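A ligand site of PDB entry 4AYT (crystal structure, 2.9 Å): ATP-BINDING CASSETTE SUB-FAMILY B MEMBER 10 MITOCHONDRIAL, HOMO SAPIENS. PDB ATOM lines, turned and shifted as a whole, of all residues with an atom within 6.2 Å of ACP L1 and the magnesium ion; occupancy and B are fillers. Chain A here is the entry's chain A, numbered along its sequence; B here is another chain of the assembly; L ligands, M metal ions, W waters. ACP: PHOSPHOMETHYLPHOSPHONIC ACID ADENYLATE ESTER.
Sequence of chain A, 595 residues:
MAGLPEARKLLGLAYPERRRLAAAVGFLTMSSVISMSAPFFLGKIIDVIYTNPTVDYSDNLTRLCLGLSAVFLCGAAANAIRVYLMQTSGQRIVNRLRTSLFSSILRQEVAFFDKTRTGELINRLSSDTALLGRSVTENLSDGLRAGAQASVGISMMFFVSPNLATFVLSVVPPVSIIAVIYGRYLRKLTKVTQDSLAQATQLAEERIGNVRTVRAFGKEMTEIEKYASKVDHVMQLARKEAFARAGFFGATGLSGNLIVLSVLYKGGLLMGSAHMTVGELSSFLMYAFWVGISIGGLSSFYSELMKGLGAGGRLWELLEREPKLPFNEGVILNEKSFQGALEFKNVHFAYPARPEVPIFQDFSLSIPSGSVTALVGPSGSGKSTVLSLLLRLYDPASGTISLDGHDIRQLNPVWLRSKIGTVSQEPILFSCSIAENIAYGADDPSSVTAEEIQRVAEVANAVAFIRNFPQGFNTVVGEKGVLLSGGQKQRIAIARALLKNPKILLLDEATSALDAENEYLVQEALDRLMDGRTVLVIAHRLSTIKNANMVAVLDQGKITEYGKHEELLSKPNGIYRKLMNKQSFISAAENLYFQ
The side-chain amino group of Lys 383 is in salt-bridge range of an oxygen (O1B) of ACP L1 (3.2 Å).
N of Ser 381 lies within hydrogen-bond range of O1B of ACP L1 (3.2 Å).
The side-chain hydroxyl of Thr 385 is in hydrogen-bond range of an oxygen (O2A) of ACP L1 (2.6 Å).
O1B of ACP L1 sits at hydrogen-bond distance from N of Lys 383 (3.5 Å).
The side-chain carboxylate (OD2) of Asp 114 lies within hydrogen-bond range of a nitrogen (N6) of ACP L1.
The backbone NH (N) of Gly 380 lies within hydrogen-bond range of an oxygen (O1B) of ACP L1, 3.2 Å away.
O2B of ACP L1 lies close to N of Ser 384, 3.2 Å away.
The backbone NH (N) of Gly 382 is in hydrogen-bond range of an oxygen (O1B) of ACP L1 (3.3 Å).
N of Thr 385 sits at hydrogen-bond distance from O2A of ACP L1.
Asp 508 touches the magnesium ion.
The nearest printed residue that does not touch the magnesium ion is Lys 383 (4.8 Å).
The magnesium ion is bound by O3G of ACP L1 (2.0 Å), O2B of ACP L1 (2.0 Å), OG of Ser 384 (2.1 Å) and OE1 of Gln 425 (2.2 Å).
The magnesium ion has four donor atoms within binding distance.
The side-chain hydroxyl of Tyr 394 lies within hydrogen-bond range of the side-chain carboxylate of Asp 114 (2.7 Å).
The side-chain carboxylate of Asp 114 lies within salt-bridge range of the guanidinium group of Arg 212 of chain B, 2.7 Å away.
OG of Ser 512 of chain B lies within hydrogen-bond range of O of Ser 379 of chain A, 3.1 Å away.
The side-chain amino group (NZ) of Lys 383 is in hydrogen-bond range of the side-chain hydroxyl (OG) of Ser 381.
The side-chain carboxylate (OD2) of Asp 508 lies close to the side-chain hydroxyl (OG) of Ser 384 (2.8 Å).
The backbone carbonyl oxygen (O) of Pro 378 is in hydrogen-bond range of the side-chain hydroxyl (OG) of Ser 381 (2.7 Å).
N of Gln 425 lies close to O of Asp 508 (3.4 Å).
NZ of Lys 383 sits at hydrogen-bond distance from O of Pro 378 (3.0 Å).
Tyr 351 touches ACP L1.
Ala 353 touches ACP L1.
Ile 359 touches ACP L1 (CD1 to O4', 3.6 Å).
Ser 379 of chain A touches ACP L1 (CA to O1G, 3.6 Å).
Tyr 394 touches ACP L1 (OH to N6, 3.6 Å).
Hydrophobic or aromatic side chains that line ACP L1: Tyr 351, Ala 353 and Ile 359.
Of the 23 residues printed, 13 come within 4 Å of ACP L1.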
ATOM      1  N   ASP A 114     -29.838   0.875  19.806  1.00  0.00           N
ATOM      2  CA  ASP A 114     -29.425   2.284  19.663  1.00  0.00           C
ATOM      3  C   ASP A 114     -30.419   3.231  20.335  1.00  0.00           C
ATOM      4  O   ASP A 114     -30.026   4.298  20.805  1.00  0.00           O
ATOM      5  CB  ASP A 114     -29.286   2.681  18.186  1.00  0.00           C
ATOM      6  CG  ASP A 114     -28.032   2.234  17.449  1.00  0.00           C
ATOM      7  OD1 ASP A 114     -27.248   1.449  18.018  1.00  0.00           O
ATOM      8  OD2 ASP A 114     -27.848   2.668  16.290  1.00  0.00           O
ATOM      9  N   TYR A 351     -27.217   7.181  10.568  1.00  0.00           N
ATOM     10  CA  TYR A 351     -27.501   6.345  11.753  1.00  0.00           C
ATOM     11  C   TYR A 351     -28.933   6.556  12.320  1.00  0.00           C
ATOM     12  O   TYR A 351     -29.468   7.668  12.229  1.00  0.00           O
ATOM     13  CB  TYR A 351     -26.477   6.614  12.851  1.00  0.00           C
ATOM     14  CG  TYR A 351     -25.179   5.862  12.683  1.00  0.00           C
ATOM     15  CD1 TYR A 351     -25.029   4.568  13.175  1.00  0.00           C
ATOM     16  CD2 TYR A 351     -24.050   6.496  12.189  1.00  0.00           C
ATOM     17  CE1 TYR A 351     -23.808   3.906  13.118  1.00  0.00           C
ATOM     18  CE2 TYR A 351     -22.809   5.846  12.152  1.00  0.00           C
ATOM     19  CZ  TYR A 351     -22.702   4.542  12.599  1.00  0.00           C
ATOM     20  OH  TYR A 351     -21.491   3.887  12.524  1.00  0.00           O
ATOM     21  N   PRO A 352     -29.582   5.518  12.889  1.00  0.00           N
ATOM     22  CA  PRO A 352     -30.969   5.677  13.364  1.00  0.00           C
ATOM     23  C   PRO A 352     -31.149   6.702  14.495  1.00  0.00           C
ATOM     24  O   PRO A 352     -32.155   7.413  14.472  1.00  0.00           O
ATOM     25  CB  PRO A 352     -31.354   4.269  13.824  1.00  0.00           C
ATOM     26  CG  PRO A 352     -30.408   3.371  13.126  1.00  0.00           C
ATOM     27  CD  PRO A 352     -29.125   4.126  13.059  1.00  0.00           C
ATOM     28  N   ALA A 353     -30.206   6.772  15.467  1.00  0.00           N
ATOM     29  CA  ALA A 353     -30.267   7.735  16.585  1.00  0.00           C
ATOM     30  C   ALA A 353     -30.214   9.207  16.080  1.00  0.00           C
ATOM     31  O   ALA A 353     -30.918  10.054  16.631  1.00  0.00           O
ATOM     32  CB  ALA A 353     -29.137   7.469  17.572  1.00  0.00           C
ATOM     33  N   ARG A 354     -29.424   9.486  15.019  1.00  0.00           N
ATOM     34  CA  ARG A 354     -29.302  10.804  14.402  1.00  0.00           C
ATOM     35  C   ARG A 354     -29.593  10.683  12.890  1.00  0.00           C
ATOM     36  O   ARG A 354     -28.668  10.764  12.075  1.00  0.00           O
ATOM     37  CB  ARG A 354     -27.887  11.393  14.630  1.00  0.00           C
ATOM     38  CG  ARG A 354     -27.536  11.770  16.069  1.00  0.00           C
ATOM     39  CD  ARG A 354     -26.163  12.415  16.111  1.00  0.00           C
ATOM     40  NE  ARG A 354     -25.696  12.656  17.482  1.00  0.00           N
ATOM     41  CZ  ARG A 354     -24.423  12.827  17.809  1.00  0.00           C
ATOM     42  NH1 ARG A 354     -23.472  12.777  16.886  1.00  0.00           N
ATOM     43  NH2 ARG A 354     -24.082  13.038  19.084  1.00  0.00           N
ATOM     44  N   ILE A 359     -24.027  10.016   6.874  1.00  0.00           N
ATOM     45  CA  ILE A 359     -22.697   9.434   6.998  1.00  0.00           C
ATOM     46  C   ILE A 359     -22.187   9.134   5.590  1.00  0.00           C
ATOM     47  O   ILE A 359     -21.057   9.487   5.253  1.00  0.00           O
ATOM     48  CB  ILE A 359     -22.729   8.175   7.928  1.00  0.00           C
ATOM     49  CG1 ILE A 359     -23.529   8.419   9.226  1.00  0.00           C
ATOM     50  CG2 ILE A 359     -21.317   7.610   8.185  1.00  0.00           C
ATOM     51  CD1 ILE A 359     -22.929   9.433  10.295  1.00  0.00           C
ATOM     52  N   PRO A 378     -10.717  12.083   7.016  1.00  0.00           N
ATOM     53  CA  PRO A 378     -10.586  12.870   8.254  1.00  0.00           C
ATOM     54  C   PRO A 378     -11.373  12.266   9.414  1.00  0.00           C
ATOM     55  O   PRO A 378     -12.207  11.406   9.180  1.00  0.00           O
ATOM     56  CB  PRO A 378     -11.174  14.242   7.866  1.00  0.00           C
ATOM     57  CG  PRO A 378     -11.367  14.203   6.378  1.00  0.00           C
ATOM     58  CD  PRO A 378     -11.559  12.786   6.027  1.00  0.00           C
ATOM     59  N   SER A 379     -11.106  12.698  10.668  1.00  0.00           N
ATOM     60  CA  SER A 379     -11.815  12.188  11.850  1.00  0.00           C
ATOM     61  C   SER A 379     -13.322  12.445  11.715  1.00  0.00           C
ATOM     62  O   SER A 379     -13.724  13.490  11.190  1.00  0.00           O
ATOM     63  CB  SER A 379     -11.286  12.832  13.128  1.00  0.00           C
ATOM     64  N   GLY A 380     -14.124  11.462  12.142  1.00  0.00           N
ATOM     65  CA  GLY A 380     -15.587  11.534  12.063  1.00  0.00           C
ATOM     66  C   GLY A 380     -16.179  11.531  10.663  1.00  0.00           C
ATOM     67  O   GLY A 380     -17.359  11.866  10.503  1.00  0.00           O
ATOM     68  N   SER A 381     -15.387  11.117   9.632  1.00  0.00           N
ATOM     69  CA  SER A 381     -15.822  11.054   8.226  1.00  0.00           C
ATOM     70  C   SER A 381     -16.832   9.915   7.960  1.00  0.00           C
ATOM     71  O   SER A 381     -17.566   9.986   6.954  1.00  0.00           O
ATOM     72  CB  SER A 381     -14.629  10.887   7.299  1.00  0.00           C
ATOM     73  OG  SER A 381     -13.809   9.819   7.755  1.00  0.00           O
ATOM     74  N   GLY A 382     -16.831   8.902   8.830  1.00  0.00           N
ATOM     75  CA  GLY A 382     -17.691   7.729   8.769  1.00  0.00           C
ATOM     76  C   GLY A 382     -16.982   6.491   8.276  1.00  0.00           C
ATOM     77  O   GLY A 382     -17.588   5.662   7.590  1.00  0.00           O
ATOM     78  N   LYS A 383     -15.695   6.337   8.627  1.00  0.00           N
ATOM     79  CA  LYS A 383     -14.859   5.208   8.235  1.00  0.00           C
ATOM     80  C   LYS A 383     -15.300   3.939   8.934  1.00  0.00           C
ATOM     81  O   LYS A 383     -15.488   2.934   8.272  1.00  0.00           O
ATOM     82  CB  LYS A 383     -13.364   5.481   8.497  1.00  0.00           C
ATOM     83  CG  LYS A 383     -12.770   6.652   7.706  1.00  0.00           C
ATOM     84  CD  LYS A 383     -11.277   6.925   7.990  1.00  0.00           C
ATOM     85  CE  LYS A 383     -10.900   7.312   9.418  1.00  0.00           C
ATOM     86  NZ  LYS A 383     -11.577   8.558   9.869  1.00  0.00           N
ATOM     87  N   SER A 384     -15.504   3.981  10.264  1.00  0.00           N
ATOM     88  CA  SER A 384     -15.954   2.836  11.081  1.00  0.00           C
ATOM     89  C   SER A 384     -17.347   2.313  10.676  1.00  0.00           C
ATOM     90  O   SER A 384     -17.602   1.116  10.822  1.00  0.00           O
ATOM     91  CB  SER A 384     -15.981   3.206  12.561  1.00  0.00           C
ATOM     92  OG  SER A 384     -14.673   3.439  13.067  1.00  0.00           O
ATOM     93  N   THR A 385     -18.227   3.191  10.149  1.00  0.00           N
ATOM     94  CA  THR A 385     -19.592   2.871   9.713  1.00  0.00           C
ATOM     95  C   THR A 385     -19.588   1.872   8.550  1.00  0.00           C
ATOM     96  O   THR A 385     -20.577   1.147   8.364  1.00  0.00           O
ATOM     97  CB  THR A 385     -20.352   4.151   9.346  1.00  0.00           C
ATOM     98  OG1 THR A 385     -20.238   5.092  10.423  1.00  0.00           O
ATOM     99  CG2 THR A 385     -21.848   3.912   9.075  1.00  0.00           C
ATOM    100  N   VAL A 386     -18.484   1.835   7.766  1.00  0.00           N
ATOM    101  CA  VAL A 386     -18.289   0.928   6.616  1.00  0.00           C
ATOM    102  C   VAL A 386     -18.352  -0.538   7.101  1.00  0.00           C
ATOM    103  O   VAL A 386     -19.083  -1.330   6.513  1.00  0.00           O
ATOM    104  CB  VAL A 386     -16.987   1.249   5.857  1.00  0.00           C
ATOM    105  CG1 VAL A 386     -16.699   0.232   4.771  1.00  0.00           C
ATOM    106  CG2 VAL A 386     -17.030   2.652   5.259  1.00  0.00           C
ATOM    107  N   TYR A 394     -26.820  -2.673  10.289  1.00  0.00           N
ATOM    108  CA  TYR A 394     -27.776  -1.761   9.666  1.00  0.00           C
ATOM    109  C   TYR A 394     -27.808  -2.053   8.161  1.00  0.00           C
ATOM    110  O   TYR A 394     -26.854  -2.626   7.625  1.00  0.00           O
ATOM    111  CB  TYR A 394     -27.340  -0.295   9.894  1.00  0.00           C
ATOM    112  CG  TYR A 394     -26.937   0.091  11.301  1.00  0.00           C
ATOM    113  CD1 TYR A 394     -27.877   0.578  12.200  1.00  0.00           C
ATOM    114  CD2 TYR A 394     -25.602   0.090  11.690  1.00  0.00           C
ATOM    115  CE1 TYR A 394     -27.517   0.981  13.488  1.00  0.00           C
ATOM    116  CE2 TYR A 394     -25.229   0.487  12.974  1.00  0.00           C
ATOM    117  CZ  TYR A 394     -26.179   0.946  13.863  1.00  0.00           C
ATOM    118  OH  TYR A 394     -25.839   1.317  15.135  1.00  0.00           O
ATOM    119  N   GLN A 425     -11.107  -0.828  16.869  1.00  0.00           N
ATOM    120  CA  GLN A 425     -10.199   0.192  17.385  1.00  0.00           C
ATOM    121  C   GLN A 425      -9.924  -0.194  18.829  1.00  0.00           C
ATOM    122  O   GLN A 425      -8.778  -0.468  19.211  1.00  0.00           O
ATOM    123  CB  GLN A 425     -10.822   1.602  17.259  1.00  0.00           C
ATOM    124  CG  GLN A 425     -10.869   2.173  15.827  1.00  0.00           C
ATOM    125  CD  GLN A 425     -11.440   3.588  15.729  1.00  0.00           C
ATOM    126  OE1 GLN A 425     -12.514   3.824  15.150  1.00  0.00           O
ATOM    127  NE2 GLN A 425     -10.718   4.568  16.269  1.00  0.00           N
ATOM    128  N   ASP A 508      -9.812  -1.919  11.844  1.00  0.00           N
ATOM    129  CA  ASP A 508      -9.944  -0.515  12.230  1.00  0.00           C
ATOM    130  C   ASP A 508      -8.778  -0.242  13.160  1.00  0.00           C
ATOM    131  O   ASP A 508      -8.883  -0.450  14.369  1.00  0.00           O
ATOM    132  CB  ASP A 508     -11.308  -0.231  12.875  1.00  0.00           C
ATOM    133  CG  ASP A 508     -11.879   1.119  12.524  1.00  0.00           C
ATOM    134  OD1 ASP A 508     -11.114   2.110  12.494  1.00  0.00           O
ATOM    135  OD2 ASP A 508     -13.111   1.214  12.298  1.00  0.00           O
ATOM    136  N   ILE A 538      -8.902   0.325   7.800  1.00  0.00           N
ATOM    137  CA  ILE A 538      -9.049   1.768   8.042  1.00  0.00           C
ATOM    138  C   ILE A 538      -7.671   2.134   8.556  1.00  0.00           C
ATOM    139  O   ILE A 538      -7.298   1.760   9.667  1.00  0.00           O
ATOM    140  CB  ILE A 538     -10.247   2.118   8.971  1.00  0.00           C
ATOM    141  CG1 ILE A 538     -11.575   2.104   8.184  1.00  0.00           C
ATOM    142  CG2 ILE A 538     -10.070   3.478   9.674  1.00  0.00           C
ATOM    143  CD1 ILE A 538     -12.219   0.778   8.008  1.00  0.00           C
ATOM    144  N   ARG B 212     -23.326  -5.839  19.382  1.00  0.00           N
ATOM    145  CA  ARG B 212     -22.538  -5.595  18.176  1.00  0.00           C
ATOM    146  C   ARG B 212     -21.484  -6.693  18.000  1.00  0.00           C
ATOM    147  O   ARG B 212     -21.392  -7.232  16.896  1.00  0.00           O
ATOM    148  CB  ARG B 212     -21.919  -4.192  18.216  1.00  0.00           C
ATOM    149  CG  ARG B 212     -22.837  -3.152  17.585  1.00  0.00           C
ATOM    150  CD  ARG B 212     -22.488  -1.716  17.935  1.00  0.00           C
ATOM    151  NE  ARG B 212     -23.693  -0.890  18.126  1.00  0.00           N
ATOM    152  CZ  ARG B 212     -24.423  -0.876  19.246  1.00  0.00           C
ATOM    153  NH1 ARG B 212     -24.103  -1.658  20.271  1.00  0.00           N
ATOM    154  NH2 ARG B 212     -25.496  -0.102  19.334  1.00  0.00           N
ATOM    155  N   SER B 379      -5.255  10.968  15.179  1.00  0.00           N
ATOM    156  CA  SER B 379      -6.382  10.693  16.091  1.00  0.00           C
ATOM    157  C   SER B 379      -5.900  10.004  17.369  1.00  0.00           C
ATOM    158  O   SER B 379      -4.976   9.182  17.303  1.00  0.00           O
ATOM    159  CB  SER B 379      -7.437   9.829  15.391  1.00  0.00           C
ATOM    160  N   SER B 512     -15.665  17.122  11.607  1.00  0.00           N
ATOM    161  CA  SER B 512     -16.252  15.794  11.544  1.00  0.00           C
ATOM    162  C   SER B 512     -17.717  15.888  11.110  1.00  0.00           C
ATOM    163  O   SER B 512     -18.102  15.278  10.100  1.00  0.00           O
ATOM    164  CB  SER B 512     -16.134  15.099  12.903  1.00  0.00           C
ATOM    165  OG  SER B 512     -14.832  15.231  13.453  1.00  0.00           O
ATOM    166  N   ALA B 513     -18.531  16.693  11.831  1.00  0.00           N
ATOM    167  CA  ALA B 513     -19.951  16.902  11.546  1.00  0.00           C
ATOM    168  C   ALA B 513     -20.208  18.353  11.088  1.00  0.00           C
ATOM    169  O   ALA B 513     -20.403  19.244  11.928  1.00  0.00           O
ATOM    170  CB  ALA B 513     -20.792  16.561  12.768  1.00  0.00           C
HETATM  171  PG  ACP L   1     -12.708   8.099  14.396  1.00  0.00           P
HETATM  172  O1G ACP L   1     -11.794   9.008  13.641  1.00  0.00           O
HETATM  173  O2G ACP L   1     -12.682   8.336  15.923  1.00  0.00           O
HETATM  174  O3G ACP L   1     -12.449   6.598  14.136  1.00  0.00           O
HETATM  175  PB  ACP L   1     -14.788   7.701  12.406  1.00  0.00           P
HETATM  176  O1B ACP L   1     -14.469   8.456  11.119  1.00  0.00           O
HETATM  177  O2B ACP L   1     -14.467   6.163  12.397  1.00  0.00           O
HETATM  178  C3B ACP L   1     -14.344   8.434  13.884  1.00  0.00           C
HETATM  179  PA  ACP L   1     -17.538   6.795  12.767  1.00  0.00           P
HETATM  180  O1A ACP L   1     -17.283   6.024  13.997  1.00  0.00           O
HETATM  181  O2A ACP L   1     -18.055   6.029  11.546  1.00  0.00           O
HETATM  182  O3A ACP L   1     -16.381   7.723  12.220  1.00  0.00           O
HETATM  183  O5' ACP L   1     -18.888   7.688  12.933  1.00  0.00           O
HETATM  184  C5' ACP L   1     -19.230   8.893  12.217  1.00  0.00           C
HETATM  185  C4' ACP L   1     -20.180   9.718  13.057  1.00  0.00           C
HETATM  186  O4' ACP L   1     -21.320   8.914  13.445  1.00  0.00           O
HETATM  187  C3' ACP L   1     -19.609  10.327  14.343  1.00  0.00           C
HETATM  188  O3' ACP L   1     -19.907  11.711  14.446  1.00  0.00           O
HETATM  189  C2' ACP L   1     -20.216   9.462  15.452  1.00  0.00           C
HETATM  190  O2' ACP L   1     -20.398  10.154  16.681  1.00  0.00           O
HETATM  191  C1' ACP L   1     -21.559   9.061  14.837  1.00  0.00           C
HETATM  192  N9  ACP L   1     -22.127   7.804  15.337  1.00  0.00           N
HETATM  193  C8  ACP L   1     -21.472   6.613  15.500  1.00  0.00           C
HETATM  194  N7  ACP L   1     -22.244   5.626  15.920  1.00  0.00           N
HETATM  195  C5  ACP L   1     -23.491   6.218  16.036  1.00  0.00           C
HETATM  196  C6  ACP L   1     -24.761   5.711  16.391  1.00  0.00           C
HETATM  197  N6  ACP L   1     -24.975   4.435  16.727  1.00  0.00           N
HETATM  198  N1  ACP L   1     -25.808   6.556  16.384  1.00  0.00           N
HETATM  199  C2  ACP L   1     -25.602   7.847  16.052  1.00  0.00           C
HETATM  200  N3  ACP L   1     -24.458   8.432  15.692  1.00  0.00           N
HETATM  201  C4  ACP L   1     -23.432   7.564  15.693  1.00  0.00           C
HETATM  202  PG  ACP L   2      -9.979  12.868  18.622  1.00  0.00           P
HETATM  203  O1G ACP L   2      -9.146  12.705  17.382  1.00  0.00           O
HETATM  204  O2G ACP L   2     -11.306  12.077  18.545  1.00  0.00           O
HETATM  205  O3G ACP L   2     -10.311  14.347  18.952  1.00  0.00           O
HETATM  206  PB  ACP L   2      -7.902  13.268  20.599  1.00  0.00           P
HETATM  207  O1B ACP L   2      -6.522  13.235  19.963  1.00  0.00           O
HETATM  208  O2B ACP L   2      -8.482  14.686  20.912  1.00  0.00           O
HETATM  209  C3B ACP L   2      -9.081  12.216  19.965  1.00  0.00           C
HETATM  210  PA  ACP L   2      -8.029  12.941  23.505  1.00  0.00           P
HETATM  211  O1A ACP L   2      -9.482  13.201  23.608  1.00  0.00           O
HETATM  212  O2A ACP L   2      -7.085  13.896  24.229  1.00  0.00           O
HETATM  213  O3A ACP L   2      -7.417  12.770  22.054  1.00  0.00           O
HETATM  214  O5' ACP L   2      -7.613  11.652  24.396  1.00  0.00           O
HETATM  215  C5' ACP L   2      -6.480  10.785  24.199  1.00  0.00           C
HETATM  216  C4' ACP L   2      -6.795   9.423  24.790  1.00  0.00           C
HETATM  217  O4' ACP L   2      -7.219   9.555  26.166  1.00  0.00           O
HETATM  218  C3' ACP L   2      -7.866   8.602  24.071  1.00  0.00           C
HETATM  219  O3' ACP L   2      -7.419   7.274  23.815  1.00  0.00           O
HETATM  220  C2' ACP L   2      -9.071   8.683  25.023  1.00  0.00           C
HETATM  221  O2' ACP L   2      -9.921   7.550  24.959  1.00  0.00           O
HETATM  222  C1' ACP L   2      -8.398   8.805  26.381  1.00  0.00           C
HETATM  223  N9  ACP L   2      -9.189   9.478  27.412  1.00  0.00           N
HETATM  224  C8  ACP L   2      -9.869  10.657  27.296  1.00  0.00           C
HETATM  225  N7  ACP L   2     -10.445  11.066  28.399  1.00  0.00           N
HETATM  226  C5  ACP L   2     -10.118  10.082  29.323  1.00  0.00           C
HETATM  227  C6  ACP L   2     -10.387   9.941  30.694  1.00  0.00           C
HETATM  228  N6  ACP L   2     -11.097  10.827  31.407  1.00  0.00           N
HETATM  229  N1  ACP L   2      -9.887   8.849  31.330  1.00  0.00           N
HETATM  230  C2  ACP L   2      -9.182   7.965  30.626  1.00  0.00           C
HETATM  231  N3  ACP L   2      -8.852   7.991  29.326  1.00  0.00           N
HETATM  232  C4  ACP L   2      -9.347   9.089  28.726  1.00  0.00           C
HETATM  233 MG    MG M   1     -13.153   4.934  13.309  1.00  0.00          MG
HETATM  234  O   HOH W   1     -24.657  10.514  13.776  1.00  0.00           O
